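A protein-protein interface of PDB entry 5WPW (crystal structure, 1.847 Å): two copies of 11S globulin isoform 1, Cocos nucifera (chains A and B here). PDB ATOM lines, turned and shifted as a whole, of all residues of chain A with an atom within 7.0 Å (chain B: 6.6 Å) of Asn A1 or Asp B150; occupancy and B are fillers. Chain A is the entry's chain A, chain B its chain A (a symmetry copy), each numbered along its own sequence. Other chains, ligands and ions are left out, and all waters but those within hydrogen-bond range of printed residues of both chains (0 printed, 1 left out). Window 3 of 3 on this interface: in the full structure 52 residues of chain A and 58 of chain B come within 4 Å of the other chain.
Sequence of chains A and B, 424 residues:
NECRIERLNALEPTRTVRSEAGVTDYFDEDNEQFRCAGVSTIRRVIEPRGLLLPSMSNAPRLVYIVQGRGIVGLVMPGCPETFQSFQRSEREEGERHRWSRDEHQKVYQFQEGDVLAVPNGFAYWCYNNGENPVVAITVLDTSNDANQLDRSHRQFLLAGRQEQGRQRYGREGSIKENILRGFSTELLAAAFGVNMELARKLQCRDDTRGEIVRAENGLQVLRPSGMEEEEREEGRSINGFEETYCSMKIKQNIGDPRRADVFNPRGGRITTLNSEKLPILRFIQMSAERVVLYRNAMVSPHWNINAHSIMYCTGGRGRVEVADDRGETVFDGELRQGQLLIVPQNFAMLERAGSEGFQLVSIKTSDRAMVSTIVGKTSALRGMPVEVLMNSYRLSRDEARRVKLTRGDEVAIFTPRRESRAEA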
ATOM      1  N   ASN A   1      32.994  -4.634  -2.858  1.00  0.00           N
ATOM      2  CA  ASN A   1      32.222  -5.770  -3.355  1.00  0.00           C
ATOM      3  C   ASN A   1      32.632  -6.114  -4.788  1.00  0.00           C
ATOM      4  O   ASN A   1      32.978  -5.230  -5.577  1.00  0.00           O
ATOM      5  CB  ASN A   1      30.717  -5.479  -3.296  1.00  0.00           C
ATOM      6  CG  ASN A   1      30.137  -5.593  -1.882  1.00  0.00           C
ATOM      7  OD1 ASN A   1      29.990  -4.592  -1.178  1.00  0.00           O
ATOM      8  ND2 ASN A   1      29.778  -6.812  -1.480  1.00  0.00           N
ATOM      9  N   GLU A   2      32.587  -7.409  -5.110  1.00  0.00           N
ATOM     10  CA  GLU A   2      32.998  -7.944  -6.403  1.00  0.00           C
ATOM     11  C   GLU A   2      31.868  -7.982  -7.422  1.00  0.00           C
ATOM     12  O   GLU A   2      31.999  -8.672  -8.442  1.00  0.00           O
ATOM     13  CB  GLU A   2      33.561  -9.367  -6.240  1.00  0.00           C
ATOM     14  CG  GLU A   2      34.989  -9.453  -5.726  1.00  0.00           C
ATOM     15  CD  GLU A   2      35.068  -9.407  -4.209  1.00  0.00           C
ATOM     16  OE1 GLU A   2      34.087  -8.960  -3.573  1.00  0.00           O
ATOM     17  OE2 GLU A   2      36.111  -9.817  -3.650  1.00  0.00           O
ATOM     18  N   CYS A   3      30.758  -7.289  -7.178  1.00  0.00           N
ATOM     19  CA  CYS A   3      29.636  -7.425  -8.097  1.00  0.00           C
ATOM     20  C   CYS A   3      29.760  -6.534  -9.321  1.00  0.00           C
ATOM     21  O   CYS A   3      28.840  -6.514 -10.150  1.00  0.00           O
ATOM     22  CB  CYS A   3      28.313  -7.169  -7.368  1.00  0.00           C
ATOM     23  SG  CYS A   3      27.768  -8.561  -6.332  1.00  0.00           S
ATOM     24  N   ARG A   4      30.869  -5.811  -9.472  1.00  0.00           N
ATOM     25  CA  ARG A   4      31.195  -5.192 -10.757  1.00  0.00           C
ATOM     26  C   ARG A   4      31.984  -6.199 -11.598  1.00  0.00           C
ATOM     27  O   ARG A   4      33.200  -6.104 -11.805  1.00  0.00           O
ATOM     28  CB  ARG A   4      31.951  -3.885 -10.560  1.00  0.00           C
ATOM     29  CG  ARG A   4      31.106  -2.765  -9.953  1.00  0.00           C
ATOM     30  CD  ARG A   4      31.906  -1.924  -8.963  1.00  0.00           C
ATOM     31  NE  ARG A   4      31.078  -1.194  -7.991  1.00  0.00           N
ATOM     32  CZ  ARG A   4      31.487  -0.884  -6.761  1.00  0.00           C
ATOM     33  NH1 ARG A   4      30.696  -0.217  -5.924  1.00  0.00           N
ATOM     34  NH2 ARG A   4      32.703  -1.252  -6.369  1.00  0.00           N
ATOM     35  N   ILE A   5      31.260  -7.194 -12.077  1.00  0.00           N
ATOM     36  CA  ILE A   5      31.847  -8.281 -12.842  1.00  0.00           C
ATOM     37  C   ILE A   5      31.845  -7.896 -14.309  1.00  0.00           C
ATOM     38  O   ILE A   5      30.796  -7.556 -14.869  1.00  0.00           O
ATOM     39  CB  ILE A   5      31.082  -9.595 -12.619  1.00  0.00           C
ATOM     40  CG1 ILE A   5      30.699  -9.761 -11.148  1.00  0.00           C
ATOM     41  CG2 ILE A   5      31.912 -10.773 -13.087  1.00  0.00           C
ATOM     42  CD1 ILE A   5      29.318  -9.239 -10.853  1.00  0.00           C
ATOM     43  N   ARG A  35      31.991 -14.692  -4.736  1.00  0.00           N
ATOM     44  CA  ARG A  35      32.100 -13.571  -3.821  1.00  0.00           C
ATOM     45  C   ARG A  35      31.008 -12.533  -4.079  1.00  0.00           C
ATOM     46  O   ARG A  35      30.513 -11.915  -3.136  1.00  0.00           O
ATOM     47  CB  ARG A  35      33.498 -12.949  -3.914  1.00  0.00           C
ATOM     48  CG  ARG A  35      34.532 -13.638  -3.006  1.00  0.00           C
ATOM     49  CD  ARG A  35      35.833 -12.849  -2.906  1.00  0.00           C
ATOM     50  NE  ARG A  35      36.551 -12.818  -4.179  1.00  0.00           N
ATOM     51  CZ  ARG A  35      37.871 -12.693  -4.300  1.00  0.00           C
ATOM     52  NH1 ARG A  35      38.640 -12.590  -3.220  1.00  0.00           N
ATOM     53  NH2 ARG A  35      38.425 -12.679  -5.512  1.00  0.00           N
ATOM     54  N   CYS A  36      30.591 -12.344  -5.331  1.00  0.00           N
ATOM     55  CA  CYS A  36      29.484 -11.425  -5.559  1.00  0.00           C
ATOM     56  C   CYS A  36      28.186 -12.001  -5.015  1.00  0.00           C
ATOM     57  O   CYS A  36      27.394 -11.282  -4.405  1.00  0.00           O
ATOM     58  CB  CYS A  36      29.340 -11.096  -7.045  1.00  0.00           C
ATOM     59  SG  CYS A  36      27.769 -10.235  -7.496  1.00  0.00           S
ATOM     60  N   ARG A 151      32.995 -14.445   6.035  1.00  0.00           N
ATOM     61  CA  ARG A 151      32.245 -14.808   4.831  1.00  0.00           C
ATOM     62  C   ARG A 151      32.945 -15.949   4.082  1.00  0.00           C
ATOM     63  O   ARG A 151      33.360 -15.825   2.935  1.00  0.00           O
ATOM     64  CB  ARG A 151      32.080 -13.596   3.918  1.00  0.00           C
ATOM     65  CG  ARG A 151      30.885 -12.699   4.192  1.00  0.00           C
ATOM     66  CD  ARG A 151      30.339 -12.071   2.866  1.00  0.00           C
ATOM     67  NE  ARG A 151      31.410 -11.790   1.902  1.00  0.00           N
ATOM     68  CZ  ARG A 151      31.264 -11.736   0.575  1.00  0.00           C
ATOM     69  NH1 ARG A 151      30.080 -11.939   0.012  1.00  0.00           N
ATOM     70  NH2 ARG A 151      32.316 -11.476  -0.194  1.00  0.00           N
ATOM     71  N   HIS A 308      20.160 -13.268  -5.891  1.00  0.00           N
ATOM     72  CA  HIS A 308      21.025 -13.891  -6.881  1.00  0.00           C
ATOM     73  C   HIS A 308      20.514 -15.298  -7.157  1.00  0.00           C
ATOM     74  O   HIS A 308      19.859 -15.917  -6.310  1.00  0.00           O
ATOM     75  CB  HIS A 308      22.481 -13.992  -6.413  1.00  0.00           C
ATOM     76  CG  HIS A 308      23.072 -12.710  -5.902  1.00  0.00           C
ATOM     77  ND1 HIS A 308      23.297 -11.615  -6.707  1.00  0.00           N
ATOM     78  CD2 HIS A 308      23.527 -12.372  -4.673  1.00  0.00           C
ATOM     79  CE1 HIS A 308      23.841 -10.647  -5.993  1.00  0.00           C
ATOM     80  NE2 HIS A 308      23.988 -11.080  -4.755  1.00  0.00           N
ATOM     81  N   ASN B  58      18.718  -1.425  -8.484  1.00  0.00           N
ATOM     82  CA  ASN B  58      19.065  -2.423  -7.469  1.00  0.00           C
ATOM     83  C   ASN B  58      18.725  -1.971  -6.056  1.00  0.00           C
ATOM     84  O   ASN B  58      18.795  -2.794  -5.137  1.00  0.00           O
ATOM     85  CB  ASN B  58      20.561  -2.752  -7.529  1.00  0.00           C
ATOM     86  CG  ASN B  58      21.463  -1.557  -7.103  1.00  0.00           C
ATOM     87  OD1 ASN B  58      21.183  -0.393  -7.431  1.00  0.00           O
ATOM     88  ND2 ASN B  58      22.547  -1.851  -6.380  1.00  0.00           N
ATOM     89  N   THR B 142      21.279   2.390  -1.223  1.00  0.00           N
ATOM     90  CA  THR B 142      22.127   1.343  -1.772  1.00  0.00           C
ATOM     91  C   THR B 142      22.754   0.465  -0.699  1.00  0.00           C
ATOM     92  O   THR B 142      23.393  -0.541  -1.038  1.00  0.00           O
ATOM     93  CB  THR B 142      23.213   1.972  -2.637  1.00  0.00           C
ATOM     94  OG1 THR B 142      23.881   2.986  -1.875  1.00  0.00           O
ATOM     95  CG2 THR B 142      22.578   2.642  -3.881  1.00  0.00           C
ATOM     96  N   SER B 143      22.612   0.840   0.570  1.00  0.00           N
ATOM     97  CA  SER B 143      22.968   0.002   1.712  1.00  0.00           C
ATOM     98  C   SER B 143      21.818  -0.885   2.179  1.00  0.00           C
ATOM     99  O   SER B 143      22.010  -1.717   3.080  1.00  0.00           O
ATOM    100  CB  SER B 143      23.408   0.889   2.882  1.00  0.00           C
ATOM    101  OG  SER B 143      24.758   1.251   2.725  1.00  0.00           O
ATOM    102  N   ASN B 147      19.279  -4.680  -1.592  1.00  0.00           N
ATOM    103  CA  ASN B 147      20.295  -4.607  -2.636  1.00  0.00           C
ATOM    104  C   ASN B 147      21.397  -5.606  -2.322  1.00  0.00           C
ATOM    105  O   ASN B 147      22.197  -5.384  -1.415  1.00  0.00           O
ATOM    106  CB  ASN B 147      20.868  -3.198  -2.706  1.00  0.00           C
ATOM    107  CG  ASN B 147      22.149  -3.137  -3.545  1.00  0.00           C
ATOM    108  OD1 ASN B 147      22.278  -3.844  -4.544  1.00  0.00           O
ATOM    109  ND2 ASN B 147      23.085  -2.287  -3.151  1.00  0.00           N
ATOM    110  N   GLN B 148      21.447  -6.710  -3.053  1.00  0.00           N
ATOM    111  CA  GLN B 148      22.491  -7.698  -2.844  1.00  0.00           C
ATOM    112  C   GLN B 148      23.654  -7.540  -3.824  1.00  0.00           C
ATOM    113  O   GLN B 148      24.548  -8.385  -3.831  1.00  0.00           O
ATOM    114  CB  GLN B 148      21.910  -9.112  -2.928  1.00  0.00           C
ATOM    115  CG  GLN B 148      20.669  -9.344  -2.050  1.00  0.00           C
ATOM    116  CD  GLN B 148      20.307 -10.824  -1.924  1.00  0.00           C
ATOM    117  OE1 GLN B 148      21.136 -11.689  -2.170  1.00  0.00           O
ATOM    118  NE2 GLN B 148      19.069 -11.107  -1.530  1.00  0.00           N
ATOM    119  N   LEU B 149      23.667  -6.480  -4.639  1.00  0.00           N
ATOM    120  CA  LEU B 149      24.845  -6.151  -5.443  1.00  0.00           C
ATOM    121  C   LEU B 149      25.817  -5.286  -4.654  1.00  0.00           C
ATOM    122  O   LEU B 149      25.852  -5.357  -3.420  1.00  0.00           O
ATOM    123  CB  LEU B 149      24.438  -5.464  -6.744  1.00  0.00           C
ATOM    124  CG  LEU B 149      23.458  -6.219  -7.631  1.00  0.00           C
ATOM    125  CD1 LEU B 149      23.032  -5.385  -8.816  1.00  0.00           C
ATOM    126  CD2 LEU B 149      24.056  -7.562  -8.091  1.00  0.00           C
ATOM    127  N   ASP B 150      26.615  -4.471  -5.340  1.00  0.00           N
ATOM    128  CA  ASP B 150      27.538  -3.580  -4.650  1.00  0.00           C
ATOM    129  C   ASP B 150      26.794  -2.361  -4.097  1.00  0.00           C
ATOM    130  O   ASP B 150      25.654  -2.069  -4.470  1.00  0.00           O
ATOM    131  CB  ASP B 150      28.665  -3.140  -5.592  1.00  0.00           C
ATOM    132  CG  ASP B 150      28.154  -2.791  -6.984  1.00  0.00           C
ATOM    133  OD1 ASP B 150      27.505  -3.648  -7.616  1.00  0.00           O
ATOM    134  OD2 ASP B 150      28.393  -1.662  -7.445  1.00  0.00           O
ATOM    135  N   ARG B 151      27.469  -1.629  -3.207  1.00  0.00           N
ATOM    136  CA  ARG B 151      26.920  -0.424  -2.582  1.00  0.00           C
ATOM    137  C   ARG B 151      27.054   0.779  -3.522  1.00  0.00           C
ATOM    138  O   ARG B 151      27.707   1.775  -3.228  1.00  0.00           O
ATOM    139  CB  ARG B 151      27.621  -0.143  -1.256  1.00  0.00           C
ATOM    140  CG  ARG B 151      27.055  -0.836  -0.028  1.00  0.00           C
ATOM    141  CD  ARG B 151      27.223   0.055   1.246  1.00  0.00           C
ATOM    142  NE  ARG B 151      28.459   0.846   1.212  1.00  0.00           N
ATOM    143  CZ  ARG B 151      28.653   2.007   1.844  1.00  0.00           C
ATOM    144  NH1 ARG B 151      27.694   2.548   2.586  1.00  0.00           N
ATOM    145  NH2 ARG B 151      29.820   2.633   1.731  1.00  0.00           N
ATOM    146  N   SER B 152      26.444   0.659  -4.694  1.00  0.00           N
ATOM    147  CA  SER B 152      26.361   1.779  -5.626  1.00  0.00           C
ATOM    148  C   SER B 152      25.045   1.648  -6.365  1.00  0.00           C
ATOM    149  O   SER B 152      24.436   0.575  -6.371  1.00  0.00           O
ATOM    150  CB  SER B 152      27.546   1.807  -6.599  1.00  0.00           C
ATOM    151  OG  SER B 152      27.335   0.939  -7.705  1.00  0.00           O
ATOM    152  N   HIS B 153      24.607   2.748  -6.978  1.00  0.00           N
ATOM    153  CA  HIS B 153      23.365   2.763  -7.745  1.00  0.00           C
ATOM    154  C   HIS B 153      23.571   2.102  -9.106  1.00  0.00           C
ATOM    155  O   HIS B 153      24.230   2.669  -9.982  1.00  0.00           O
ATOM    156  CB  HIS B 153      22.864   4.185  -7.954  1.00  0.00           C
ATOM    157  CG  HIS B 153      21.597   4.241  -8.746  1.00  0.00           C
ATOM    158  ND1 HIS B 153      21.261   5.305  -9.554  1.00  0.00           N
ATOM    159  CD2 HIS B 153      20.590   3.346  -8.862  1.00  0.00           C
ATOM    160  CE1 HIS B 153      20.088   5.075 -10.116  1.00  0.00           C
ATOM    161  NE2 HIS B 153      19.665   3.888  -9.723  1.00  0.00           N
ATOM    162  N   ARG B 154      22.995   0.916  -9.300  1.00  0.00           N
ATOM    163  CA  ARG B 154      22.985   0.250 -10.597  1.00  0.00           C
ATOM    164  C   ARG B 154      21.586   0.417 -11.183  1.00  0.00           C
ATOM    165  O   ARG B 154      20.609  -0.123 -10.642  1.00  0.00           O
ATOM    166  CB  ARG B 154      23.352  -1.235 -10.486  1.00  0.00           C
ATOM    167  CG  ARG B 154      24.411  -1.611  -9.429  1.00  0.00           C
ATOM    168  CD  ARG B 154      25.825  -1.812 -10.001  1.00  0.00           C
ATOM    169  NE  ARG B 154      25.862  -2.699 -11.171  1.00  0.00           N
ATOM    170  CZ  ARG B 154      26.461  -3.888 -11.228  1.00  0.00           C
ATOM    171  NH1 ARG B 154      27.103  -4.384 -10.180  1.00  0.00           N
ATOM    172  NH2 ARG B 154      26.431  -4.582 -12.361  1.00  0.00           N
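Asn A1 touches just one residue of chain B: Asp B150 (3.9 Å). Arg A151 touches none of the printed residues of chain B. Of the printed residues of chain A, Gln B148 touches His A308 (2.9 Å). Printed residues of chain A within 4 Å of Leu B149: Cys A3 (3.9 Å) and His A308 (3.7 Å). Of chain A, only Asn A1, Cys A3 and Arg A4 come within 4 Å of Asp B150. Printed residues of chain A within 4 Å of Ser B152: Arg A4 (3.8 Å). Of the printed residues of chain A, Arg B154 touches Cys A3 (2.7 Å). The nearest residue of chain B that does not touch Asn A1 is Arg B151 (4.4 Å). The nearest printed residue of chain B that does not touch Arg A4 is Arg B154 (4.1 Å).
The backbone carbonyl oxygen (O) of Gln B148 lies within hydrogen-bond range of a ring nitrogen (NE2) of His A308 (2.9 Å). The guanidinium group (NE) of Arg A4 lies within salt-bridge range of the side-chain carboxylate (OD2) of Asp B150 (2.8 Å). NH1 of Arg B154 lies within hydrogen-bond range of O of Cys A3, 2.7 Å away.
Position printed for both chains: 151.
OD2 of Asp B150 lies within hydrogen-bond range of OG of Ser B152 (2.8 Å). OD1 of Asn B147 lies within hydrogen-bond range of N of Leu B149 (3.0 Å). ND2 of Asn B147 lies within hydrogen-bond range of O of Asp B150, 2.9 Å away. OD1 of Asn B58 sits at hydrogen-bond distance from N of Arg B154 (2.9 Å). ND2 of Asn B58 is in hydrogen-bond range of O of Ser B152 (3.1 Å). SG of Cys A3 forms a disulfide with SG of Cys A36, 2.0 Å away.
Of the 9 printed residues of chain A, 4 touch a printed residue of chain B. Printed residues of chain A that touch a printed residue of chain B: Asn A1, Cys A3, Arg A4 and His A308. Hydrophobic or aromatic side chains of chain B that line the printed part of chain A: Leu B149. Among the printed residues, 8 pairs touch across the chains. Among the printed residues, Asp or Glu carboxylates within 4 Å of a Lys or Arg side-chain nitrogen of the other chain: Arg A4 with Asp B150 (2.8 Å).
Asp B150 touches Asn A1. Cys A3 touches Leu B149. Cys A3 touches Asp B150. Arg A4 touches Ser B152 (NH1 to CB, 3.8 Å). CE1 of His A308 touches CD2 of Leu B149, at 3.7 Å.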
